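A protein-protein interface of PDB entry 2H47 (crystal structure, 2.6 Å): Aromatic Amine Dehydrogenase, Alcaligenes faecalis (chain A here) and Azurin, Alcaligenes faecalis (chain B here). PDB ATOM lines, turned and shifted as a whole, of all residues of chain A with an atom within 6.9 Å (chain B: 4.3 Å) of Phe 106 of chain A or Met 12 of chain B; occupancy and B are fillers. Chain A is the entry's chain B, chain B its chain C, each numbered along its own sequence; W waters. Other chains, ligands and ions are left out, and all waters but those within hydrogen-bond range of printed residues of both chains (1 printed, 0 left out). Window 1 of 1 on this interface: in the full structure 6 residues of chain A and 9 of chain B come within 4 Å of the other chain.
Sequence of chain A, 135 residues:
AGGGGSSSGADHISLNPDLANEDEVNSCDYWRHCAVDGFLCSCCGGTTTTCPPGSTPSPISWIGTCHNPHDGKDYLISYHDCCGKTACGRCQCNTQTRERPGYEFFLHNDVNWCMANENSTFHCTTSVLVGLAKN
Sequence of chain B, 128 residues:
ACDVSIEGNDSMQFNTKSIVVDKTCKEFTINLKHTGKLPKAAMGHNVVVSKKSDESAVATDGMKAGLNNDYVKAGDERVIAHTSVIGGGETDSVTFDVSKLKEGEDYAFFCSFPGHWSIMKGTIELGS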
ATOM      1  N   PRO A  59      14.503  30.224 -20.471  1.00  0.00           N
ATOM      2  CA  PRO A  59      14.915  29.893 -21.838  1.00  0.00           C
ATOM      3  C   PRO A  59      13.798  29.214 -22.617  1.00  0.00           C
ATOM      4  O   PRO A  59      13.665  29.413 -23.821  1.00  0.00           O
ATOM      5  CB  PRO A  59      16.118  28.983 -21.621  1.00  0.00           C
ATOM      6  CG  PRO A  59      15.749  28.265 -20.365  1.00  0.00           C
ATOM      7  CD  PRO A  59      15.216  29.382 -19.495  1.00  0.00           C
ATOM      8  N   ILE A  60      12.995  28.412 -21.927  1.00  0.00           N
ATOM      9  CA  ILE A  60      11.896  27.723 -22.581  1.00  0.00           C
ATOM     10  C   ILE A  60      10.606  28.507 -22.376  1.00  0.00           C
ATOM     11  O   ILE A  60      10.626  29.591 -21.795  1.00  0.00           O
ATOM     12  CB  ILE A  60      11.740  26.291 -22.045  1.00  0.00           C
ATOM     13  CG1 ILE A  60      11.439  26.313 -20.549  1.00  0.00           C
ATOM     14  CG2 ILE A  60      13.021  25.518 -22.294  1.00  0.00           C
ATOM     15  CD1 ILE A  60      11.315  24.928 -19.931  1.00  0.00           C
ATOM     16  N   SER A  61       9.493  27.967 -22.858  1.00  0.00           N
ATOM     17  CA  SER A  61       8.206  28.643 -22.731  1.00  0.00           C
ATOM     18  C   SER A  61       7.127  27.868 -23.467  1.00  0.00           C
ATOM     19  O   SER A  61       7.424  26.924 -24.192  1.00  0.00           O
ATOM     20  CB  SER A  61       8.281  30.038 -23.348  1.00  0.00           C
ATOM     21  OG  SER A  61       8.345  29.953 -24.765  1.00  0.00           O
ATOM     22  N   TRQ A  62       5.874  28.258 -23.268  1.00  0.00           N
ATOM     23  CA  TRQ A  62       4.783  27.614 -23.983  1.00  0.00           C
ATOM     24  C   TRQ A  62       4.399  28.596 -25.093  1.00  0.00           C
ATOM     25  O   TRQ A  62       4.607  29.801 -24.961  1.00  0.00           O
ATOM     26  CB  TRQ A  62       3.615  27.282 -23.037  1.00  0.00           C
ATOM     27  CG  TRQ A  62       2.971  28.428 -22.309  1.00  0.00           C
ATOM     28  CD1 TRQ A  62       1.956  29.209 -22.791  1.00  0.00           C
ATOM     29  NE1 TRQ A  62       1.564  30.124 -21.852  1.00  0.00           N
ATOM     30  CE2 TRQ A  62       2.334  29.965 -20.727  1.00  0.00           C
ATOM     31  CZ2 TRQ A  62       2.285  30.679 -19.523  1.00  0.00           C
ATOM     32  CH2 TRQ A  62       3.171  30.324 -18.536  1.00  0.00           C
ATOM     33  CZ3 TRQ A  62       4.091  29.274 -18.717  1.00  0.00           C
ATOM     34  CE3 TRQ A  62       4.146  28.560 -19.915  1.00  0.00           C
ATOM     35  CD2 TRQ A  62       3.248  28.900 -20.962  1.00  0.00           C
ATOM     36  O6  TRQ A  62       3.022  31.009 -17.527  1.00  0.00           O
ATOM     37  O7  TRQ A  62       1.473  31.612 -19.394  1.00  0.00           O
ATOM     38  N   ILE A  63       3.876  28.092 -26.201  1.00  0.00           N
ATOM     39  CA  ILE A  63       3.539  28.966 -27.321  1.00  0.00           C
ATOM     40  C   ILE A  63       2.057  29.071 -27.687  1.00  0.00           C
ATOM     41  O   ILE A  63       1.301  28.102 -27.607  1.00  0.00           O
ATOM     42  CB  ILE A  63       4.362  28.553 -28.584  1.00  0.00           C
ATOM     43  CG1 ILE A  63       5.818  28.991 -28.415  1.00  0.00           C
ATOM     44  CG2 ILE A  63       3.784  29.173 -29.832  1.00  0.00           C
ATOM     45  CD1 ILE A  63       6.781  27.854 -28.191  1.00  0.00           C
ATOM     46  N   GLY A  64       1.653  30.269 -28.089  1.00  0.00           N
ATOM     47  CA  GLY A  64       0.276  30.487 -28.481  1.00  0.00           C
ATOM     48  C   GLY A  64       0.145  31.088 -29.874  1.00  0.00           C
ATOM     49  O   GLY A  64       1.086  31.694 -30.402  1.00  0.00           O
ATOM     50  N   HIS A  80       7.400  33.293 -22.272  1.00  0.00           N
ATOM     51  CA  HIS A  80       8.536  33.036 -21.394  1.00  0.00           C
ATOM     52  C   HIS A  80       8.231  33.533 -19.982  1.00  0.00           C
ATOM     53  O   HIS A  80       7.655  34.605 -19.802  1.00  0.00           O
ATOM     54  CB  HIS A  80       9.774  33.763 -21.916  1.00  0.00           C
ATOM     55  CG  HIS A  80      10.377  33.147 -23.137  1.00  0.00           C
ATOM     56  ND1 HIS A  80      11.147  32.005 -23.093  1.00  0.00           N
ATOM     57  CD2 HIS A  80      10.333  33.520 -24.438  1.00  0.00           C
ATOM     58  CE1 HIS A  80      11.553  31.703 -24.312  1.00  0.00           C
ATOM     59  NE2 HIS A  80      11.073  32.607 -25.147  1.00  0.00           N
ATOM     60  N   ARG A 100      -3.318  23.555 -25.541  1.00  0.00           N
ATOM     61  CA  ARG A 100      -3.572  22.122 -25.568  1.00  0.00           C
ATOM     62  C   ARG A 100      -2.928  21.361 -24.410  1.00  0.00           C
ATOM     63  O   ARG A 100      -2.067  21.885 -23.703  1.00  0.00           O
ATOM     64  CB  ARG A 100      -3.076  21.561 -26.901  1.00  0.00           C
ATOM     65  CG  ARG A 100      -3.768  22.173 -28.122  1.00  0.00           C
ATOM     66  CD  ARG A 100      -5.204  21.664 -28.261  1.00  0.00           C
ATOM     67  NE  ARG A 100      -5.935  22.292 -29.366  1.00  0.00           N
ATOM     68  CZ  ARG A 100      -6.373  23.552 -29.370  1.00  0.00           C
ATOM     69  NH1 ARG A 100      -6.164  24.343 -28.325  1.00  0.00           N
ATOM     70  NH2 ARG A 100      -7.021  24.029 -30.425  1.00  0.00           N
ATOM     71  N   PRO A 101      -3.348  20.106 -24.198  1.00  0.00           N
ATOM     72  CA  PRO A 101      -2.818  19.259 -23.124  1.00  0.00           C
ATOM     73  C   PRO A 101      -1.328  18.931 -23.245  1.00  0.00           C
ATOM     74  O   PRO A 101      -0.684  19.247 -24.246  1.00  0.00           O
ATOM     75  CB  PRO A 101      -3.691  18.012 -23.213  1.00  0.00           C
ATOM     76  CG  PRO A 101      -4.996  18.551 -23.715  1.00  0.00           C
ATOM     77  CD  PRO A 101      -4.531  19.476 -24.808  1.00  0.00           C
ATOM     78  N   GLY A 102      -0.801  18.277 -22.213  1.00  0.00           N
ATOM     79  CA  GLY A 102       0.609  17.913 -22.160  1.00  0.00           C
ATOM     80  C   GLY A 102       1.228  17.121 -23.301  1.00  0.00           C
ATOM     81  O   GLY A 102       2.437  17.207 -23.508  1.00  0.00           O
ATOM     82  N   TYR A 103       0.434  16.352 -24.040  1.00  0.00           N
ATOM     83  CA  TYR A 103       0.988  15.569 -25.138  1.00  0.00           C
ATOM     84  C   TYR A 103       1.434  16.446 -26.309  1.00  0.00           C
ATOM     85  O   TYR A 103       1.863  15.950 -27.349  1.00  0.00           O
ATOM     86  CB  TYR A 103      -0.001  14.482 -25.582  1.00  0.00           C
ATOM     87  CG  TYR A 103      -1.425  14.947 -25.744  1.00  0.00           C
ATOM     88  CD1 TYR A 103      -1.850  15.551 -26.929  1.00  0.00           C
ATOM     89  CD2 TYR A 103      -2.352  14.782 -24.714  1.00  0.00           C
ATOM     90  CE1 TYR A 103      -3.164  15.976 -27.086  1.00  0.00           C
ATOM     91  CE2 TYR A 103      -3.674  15.206 -24.860  1.00  0.00           C
ATOM     92  CZ  TYR A 103      -4.072  15.801 -26.051  1.00  0.00           C
ATOM     93  OH  TYR A 103      -5.371  16.211 -26.216  1.00  0.00           O
ATOM     94  N   GLU A 104       1.316  17.755 -26.113  1.00  0.00           N
ATOM     95  CA  GLU A 104       1.757  18.781 -27.065  1.00  0.00           C
ATOM     96  C   GLU A 104       2.352  19.823 -26.100  1.00  0.00           C
ATOM     97  O   GLU A 104       2.039  21.015 -26.144  1.00  0.00           O
ATOM     98  CB  GLU A 104       0.578  19.385 -27.859  1.00  0.00           C
ATOM     99  CG  GLU A 104      -0.137  18.424 -28.812  1.00  0.00           C
ATOM    100  CD  GLU A 104      -0.934  19.134 -29.917  1.00  0.00           C
ATOM    101  OE1 GLU A 104      -0.312  19.586 -30.905  1.00  0.00           O
ATOM    102  OE2 GLU A 104      -2.183  19.239 -29.799  1.00  0.00           O
ATOM    103  N   PHE A 105       3.217  19.317 -25.225  1.00  0.00           N
ATOM    104  CA  PHE A 105       3.863  20.081 -24.171  1.00  0.00           C
ATOM    105  C   PHE A 105       4.104  21.567 -24.382  1.00  0.00           C
ATOM    106  O   PHE A 105       3.762  22.368 -23.511  1.00  0.00           O
ATOM    107  CB  PHE A 105       5.177  19.403 -23.771  1.00  0.00           C
ATOM    108  CG  PHE A 105       5.519  19.563 -22.311  1.00  0.00           C
ATOM    109  CD1 PHE A 105       4.670  19.056 -21.325  1.00  0.00           C
ATOM    110  CD2 PHE A 105       6.660  20.249 -21.919  1.00  0.00           C
ATOM    111  CE1 PHE A 105       4.949  19.237 -19.972  1.00  0.00           C
ATOM    112  CE2 PHE A 105       6.948  20.435 -20.571  1.00  0.00           C
ATOM    113  CZ  PHE A 105       6.089  19.929 -19.595  1.00  0.00           C
ATOM    114  N   PHE A 106       4.674  21.959 -25.515  1.00  0.00           N
ATOM    115  CA  PHE A 106       4.951  23.381 -25.723  1.00  0.00           C
ATOM    116  C   PHE A 106       3.766  24.251 -26.134  1.00  0.00           C
ATOM    117  O   PHE A 106       3.933  25.411 -26.517  1.00  0.00           O
ATOM    118  CB  PHE A 106       6.100  23.564 -26.712  1.00  0.00           C
ATOM    119  CG  PHE A 106       7.419  23.039 -26.211  1.00  0.00           C
ATOM    120  CD1 PHE A 106       7.852  21.757 -26.551  1.00  0.00           C
ATOM    121  CD2 PHE A 106       8.225  23.821 -25.392  1.00  0.00           C
ATOM    122  CE1 PHE A 106       9.071  21.267 -26.083  1.00  0.00           C
ATOM    123  CE2 PHE A 106       9.441  23.343 -24.920  1.00  0.00           C
ATOM    124  CZ  PHE A 106       9.865  22.062 -25.267  1.00  0.00           C
ATOM    125  N   LEU A 107       2.568  23.692 -26.043  1.00  0.00           N
ATOM    126  CA  LEU A 107       1.351  24.429 -26.373  1.00  0.00           C
ATOM    127  C   LEU A 107       0.443  24.260 -25.171  1.00  0.00           C
ATOM    128  O   LEU A 107      -0.748  24.558 -25.226  1.00  0.00           O
ATOM    129  CB  LEU A 107       0.677  23.833 -27.607  1.00  0.00           C
ATOM    130  CG  LEU A 107       1.548  23.778 -28.858  1.00  0.00           C
ATOM    131  CD1 LEU A 107       0.774  23.111 -29.967  1.00  0.00           C
ATOM    132  CD2 LEU A 107       1.972  25.188 -29.255  1.00  0.00           C
ATOM    133  N   HIS A 108       1.037  23.762 -24.091  1.00  0.00           N
ATOM    134  CA  HIS A 108       0.339  23.506 -22.842  1.00  0.00           C
ATOM    135  C   HIS A 108       0.781  24.545 -21.809  1.00  0.00           C
ATOM    136  O   HIS A 108       1.971  24.843 -21.702  1.00  0.00           O
ATOM    137  CB  HIS A 108       0.695  22.100 -22.361  1.00  0.00           C
ATOM    138  CG  HIS A 108       0.020  21.701 -21.088  1.00  0.00           C
ATOM    139  ND1 HIS A 108       0.667  21.004 -20.091  1.00  0.00           N
ATOM    140  CD2 HIS A 108      -1.253  21.874 -20.661  1.00  0.00           C
ATOM    141  CE1 HIS A 108      -0.176  20.764 -19.104  1.00  0.00           C
ATOM    142  NE2 HIS A 108      -1.348  21.280 -19.426  1.00  0.00           N
ATOM    143  N   ASN A 109      -0.161  25.102 -21.050  1.00  0.00           N
ATOM    144  CA  ASN A 109       0.221  26.101 -20.057  1.00  0.00           C
ATOM    145  C   ASN A 109      -0.119  25.777 -18.607  1.00  0.00           C
ATOM    146  O   ASN A 109      -0.216  26.681 -17.775  1.00  0.00           O
ATOM    147  CB  ASN A 109      -0.351  27.480 -20.421  1.00  0.00           C
ATOM    148  CG  ASN A 109      -1.864  27.538 -20.338  1.00  0.00           C
ATOM    149  OD1 ASN A 109      -2.497  26.736 -19.655  1.00  0.00           O
ATOM    150  ND2 ASN A 109      -2.447  28.513 -21.019  1.00  0.00           N
ATOM    151  N   TRP A 113       6.728  27.191 -16.649  1.00  0.00           N
ATOM    152  CA  TRP A 113       7.769  27.290 -17.663  1.00  0.00           C
ATOM    153  C   TRP A 113       9.158  27.701 -17.163  1.00  0.00           C
ATOM    154  O   TRP A 113      10.093  27.880 -17.947  1.00  0.00           O
ATOM    155  CB  TRP A 113       7.271  28.168 -18.827  1.00  0.00           C
ATOM    156  CG  TRP A 113       6.408  27.333 -19.771  1.00  0.00           C
ATOM    157  CD1 TRP A 113       5.063  27.492 -20.067  1.00  0.00           C
ATOM    158  CD2 TRP A 113       6.810  26.113 -20.406  1.00  0.00           C
ATOM    159  NE1 TRP A 113       4.629  26.433 -20.816  1.00  0.00           N
ATOM    160  CE2 TRP A 113       5.675  25.577 -21.044  1.00  0.00           C
ATOM    161  CE3 TRP A 113       8.025  25.417 -20.492  1.00  0.00           C
ATOM    162  CZ2 TRP A 113       5.717  24.369 -21.766  1.00  0.00           C
ATOM    163  CZ3 TRP A 113       8.066  24.215 -21.208  1.00  0.00           C
ATOM    164  CH2 TRP A 113       6.917  23.707 -21.834  1.00  0.00           C
ATOM    165  N   ASN B   9      19.669  27.544 -29.644  1.00  0.00           N
ATOM    166  CA  ASN B   9      19.874  27.888 -28.239  1.00  0.00           C
ATOM    167  C   ASN B   9      18.903  27.146 -27.320  1.00  0.00           C
ATOM    168  O   ASN B   9      18.065  26.369 -27.783  1.00  0.00           O
ATOM    169  CB  ASN B   9      19.707  29.402 -28.051  1.00  0.00           C
ATOM    170  CG  ASN B   9      18.527  29.966 -28.839  1.00  0.00           C
ATOM    171  OD1 ASN B   9      17.414  29.444 -28.777  1.00  0.00           O
ATOM    172  ND2 ASN B   9      18.772  31.039 -29.584  1.00  0.00           N
ATOM    173  N   ASP B  10      19.025  27.387 -26.015  1.00  0.00           N
ATOM    174  CA  ASP B  10      18.143  26.762 -25.027  1.00  0.00           C
ATOM    175  C   ASP B  10      16.773  27.416 -25.157  1.00  0.00           C
ATOM    176  O   ASP B  10      15.850  27.110 -24.404  1.00  0.00           O
ATOM    177  CB  ASP B  10      18.643  27.011 -23.600  1.00  0.00           C
ATOM    178  CG  ASP B  10      20.106  26.693 -23.425  1.00  0.00           C
ATOM    179  OD1 ASP B  10      20.495  25.524 -23.631  1.00  0.00           O
ATOM    180  OD2 ASP B  10      20.870  27.619 -23.076  1.00  0.00           O
ATOM    181  N   SER B  11      16.657  28.321 -26.124  1.00  0.00           N
ATOM    182  CA  SER B  11      15.429  29.074 -26.348  1.00  0.00           C
ATOM    183  C   SER B  11      14.545  28.539 -27.487  1.00  0.00           C
ATOM    184  O   SER B  11      13.647  29.239 -27.957  1.00  0.00           O
ATOM    185  CB  SER B  11      15.789  30.540 -26.604  1.00  0.00           C
ATOM    186  OG  SER B  11      16.865  30.951 -25.769  1.00  0.00           O
ATOM    187  N   MET B  12      14.798  27.308 -27.915  1.00  0.00           N
ATOM    188  CA  MET B  12      14.027  26.666 -28.986  1.00  0.00           C
ATOM    189  C   MET B  12      13.937  27.530 -30.250  1.00  0.00           C
ATOM    190  O   MET B  12      12.843  27.831 -30.733  1.00  0.00           O
ATOM    191  CB  MET B  12      12.619  26.318 -28.471  1.00  0.00           C
ATOM    192  CG  MET B  12      11.893  25.229 -29.269  1.00  0.00           C
ATOM    193  SD  MET B  12      10.379  24.581 -28.472  1.00  0.00           S
ATOM    194  CE  MET B  12       9.138  24.858 -29.730  1.00  0.00           C
ATOM    195  N   GLN B  13      15.097  27.914 -30.783  1.00  0.00           N
ATOM    196  CA  GLN B  13      15.189  28.753 -31.984  1.00  0.00           C
ATOM    197  C   GLN B  13      16.312  28.372 -32.939  1.00  0.00           C
ATOM    198  O   GLN B  13      17.371  27.909 -32.517  1.00  0.00           O
ATOM    199  CB  GLN B  13      15.470  30.206 -31.622  1.00  0.00           C
ATOM    200  CG  GLN B  13      14.349  31.045 -31.104  1.00  0.00           C
ATOM    201  CD  GLN B  13      14.816  32.477 -30.942  1.00  0.00           C
ATOM    202  OE1 GLN B  13      15.859  32.732 -30.334  1.00  0.00           O
ATOM    203  NE2 GLN B  13      14.059  33.415 -31.493  1.00  0.00           N
ATOM    204  N   MET B  43      16.855  19.659 -23.494  1.00  0.00           N
ATOM    205  CA  MET B  43      16.606  20.665 -24.519  1.00  0.00           C
ATOM    206  C   MET B  43      17.690  20.592 -25.598  1.00  0.00           C
ATOM    207  O   MET B  43      18.418  21.555 -25.835  1.00  0.00           O
ATOM    208  CB  MET B  43      16.575  22.052 -23.859  1.00  0.00           C
ATOM    209  CG  MET B  43      16.308  23.231 -24.781  1.00  0.00           C
ATOM    210  SD  MET B  43      14.760  23.120 -25.674  1.00  0.00           S
ATOM    211  CE  MET B  43      13.623  23.169 -24.366  1.00  0.00           C
ATOM    212  N   PRO B 114      11.078  16.056 -29.653  1.00  0.00           N
ATOM    213  CA  PRO B 114       9.706  16.213 -29.162  1.00  0.00           C
ATOM    214  C   PRO B 114       9.183  17.634 -28.925  1.00  0.00           C
ATOM    215  O   PRO B 114       9.567  18.302 -27.958  1.00  0.00           O
ATOM    216  CB  PRO B 114       9.701  15.358 -27.901  1.00  0.00           C
ATOM    217  CG  PRO B 114      10.525  14.202 -28.329  1.00  0.00           C
ATOM    218  CD  PRO B 114      11.700  14.865 -29.043  1.00  0.00           C
ATOM    219  N   GLY B 115       8.313  18.079 -29.838  1.00  0.00           N
ATOM    220  CA  GLY B 115       7.681  19.388 -29.749  1.00  0.00           C
ATOM    221  C   GLY B 115       8.440  20.629 -30.185  1.00  0.00           C
ATOM    222  O   GLY B 115       7.964  21.744 -29.964  1.00  0.00           O
ATOM    223  N   HIS B 116       9.604  20.459 -30.805  1.00  0.00           N
ATOM    224  CA  HIS B 116      10.401  21.602 -31.243  1.00  0.00           C
ATOM    225  C   HIS B 116      10.090  22.039 -32.664  1.00  0.00           C
ATOM    226  O   HIS B 116      10.342  23.186 -33.032  1.00  0.00           O
ATOM    227  CB  HIS B 116      11.901  21.293 -31.130  1.00  0.00           C
ATOM    228  CG  HIS B 116      12.399  21.207 -29.723  1.00  0.00           C
ATOM    229  ND1 HIS B 116      13.733  21.055 -29.414  1.00  0.00           N
ATOM    230  CD2 HIS B 116      11.745  21.252 -28.535  1.00  0.00           C
ATOM    231  CE1 HIS B 116      13.881  21.012 -28.102  1.00  0.00           C
ATOM    232  NE2 HIS B 116      12.689  21.130 -27.546  1.00  0.00           N
ATOM    233  N   SER B 118       7.414  22.761 -33.880  1.00  0.00           N
ATOM    234  CA  SER B 118       6.324  23.733 -33.900  1.00  0.00           C
ATOM    235  C   SER B 118       6.849  25.115 -34.295  1.00  0.00           C
ATOM    236  O   SER B 118       6.188  25.847 -35.033  1.00  0.00           O
ATOM    237  CB  SER B 118       5.632  23.803 -32.529  1.00  0.00           C
ATOM    238  OG  SER B 118       6.499  24.292 -31.520  1.00  0.00           O
ATOM    239  N   ILE B 119       8.046  25.456 -33.817  1.00  0.00           N
ATOM    240  CA  ILE B 119       8.656  26.752 -34.118  1.00  0.00           C
ATOM    241  C   ILE B 119      10.033  26.668 -34.782  1.00  0.00           C
ATOM    242  O   ILE B 119      10.391  27.539 -35.580  1.00  0.00           O
ATOM    243  CB  ILE B 119       8.758  27.622 -32.843  1.00  0.00           C
ATOM    244  CG1 ILE B 119       7.353  27.922 -32.325  1.00  0.00           C
ATOM    245  CG2 ILE B 119       9.491  28.926 -33.142  1.00  0.00           C
ATOM    246  CD1 ILE B 119       7.321  28.930 -31.218  1.00  0.00           C
ATOM    247  N   MET B 120      10.807  25.640 -34.452  1.00  0.00           N
ATOM    248  CA  MET B 120      12.128  25.472 -35.058  1.00  0.00           C
ATOM    249  C   MET B 120      11.937  24.846 -36.433  1.00  0.00           C
ATOM    250  O   MET B 120      12.166  23.651 -36.624  1.00  0.00           O
ATOM    251  CB  MET B 120      13.012  24.572 -34.196  1.00  0.00           C
ATOM    252  CG  MET B 120      13.455  25.198 -32.893  1.00  0.00           C
ATOM    253  SD  MET B 120      14.588  24.108 -32.050  1.00  0.00           S
ATOM    254  CE  MET B 120      16.143  24.772 -32.569  1.00  0.00           C
HETATM  255  O   HOH W   1       4.981  21.098 -28.657  1.00  0.00           O
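A ring nitrogen (ND1) of His 80 of chain A lies within hydrogen-bond range of the backbone carbonyl oxygen (O) of Ile 60 of chain A, 2.8 Å away. The backbone carbonyl oxygen (O) of Phe 106 of chain A is in hydrogen-bond range of the backbone NH (N) of Ile 63 of chain A. The side-chain amide oxygen (OD1) of Asn 9 of chain B sits close to the backbone NH (N) of Ser 11 of chain B (3.0 Å). The backbone NH (N) of Met 12 of chain B lies within hydrogen-bond range of the side-chain amide oxygen (OD1) of Asn 9 of chain B (3.5 Å). The side-chain sulfur of Met 43 of chain B sits close to a ring nitrogen (NE2) of His 116 of chain B (3.4 Å). The backbone carbonyl oxygen (O) of Gly 115 of chain B lies within hydrogen-bond range of the side-chain hydroxyl (OG) of Ser 118 of chain B (3.3 Å).
Among the printed residues, pairs that only touch across the chains: Pro 59 of chain A with Ser 11 of chain B (3.1 Å), Ile 60 of chain A with Asp 10 of chain B (3.9 Å), Ile 60 of chain A with Met 43 of chain B (3.2 Å), Ile 63 of chain A with Ile 119 of chain B (3.2 Å), Phe 106 of chain A with Met 12 of chain B (3.8 Å), Phe 106 of chain A with Pro 114 of chain B (3.5 Å), Phe 106 of chain A with Gly 115 of chain B (3.4 Å) and Phe 106 of chain A with His 116 of chain B (3.6 Å).
Water W1 bridges the backbone NH (N) of Phe 106 of chain A (3.3 Å) and the backbone carbonyl oxygen (O) of Gly 115 of chain B (3.3 Å).
Of the printed residues of chain B, Phe 106 of chain A touches Met 12 (3.8 Å), Pro 114 (3.5 Å), Gly 115 (3.4 Å) and His 116 (3.6 Å). Met 12 of chain B touches just one residue of chain A: Phe 106 (3.8 Å). Printed residues of chain B within 4 Å of Pro 59 of chain A: Asp 10 (3.2 Å) and Ser 11 (3.1 Å). Of the printed residues of chain A, Ile 119 of chain B touches Ile 63 (3.2 Å). Gly 102 of chain A touches none of the printed residues of chain B. The nearest printed residue of chain B that does not touch Phe 106 of chain A is Met 43 of chain B (4.02 Å). The nearest residue of chain A that does not touch Met 12 of chain B is Ile 63 of chain A (4.1 Å). The nearest printed residue of chain A that does not touch Asp 10 of chain B is His 80 of chain A (6.3 Å).
Hydrophobic or aromatic side chains of chain B that line the printed part of chain A: Met 12, Met 43, His 116 and Ile 119. Hydrophobic or aromatic side chains of chain A that line the printed part of chain B: Pro 59, Ile 60, Ile 63 and Phe 106. Among the printed residues, 9 pairs touch across the chains. Among the printed residues, no Asp or Glu carboxylate lies within 4 Å of a Lys or Arg side-chain nitrogen of the other chain.
The backbone carbonyl oxygen (O) of Asp 10 of chain B sits close to the backbone carbonyl oxygen (O) of Pro 59 of chain A (3.2 Å).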
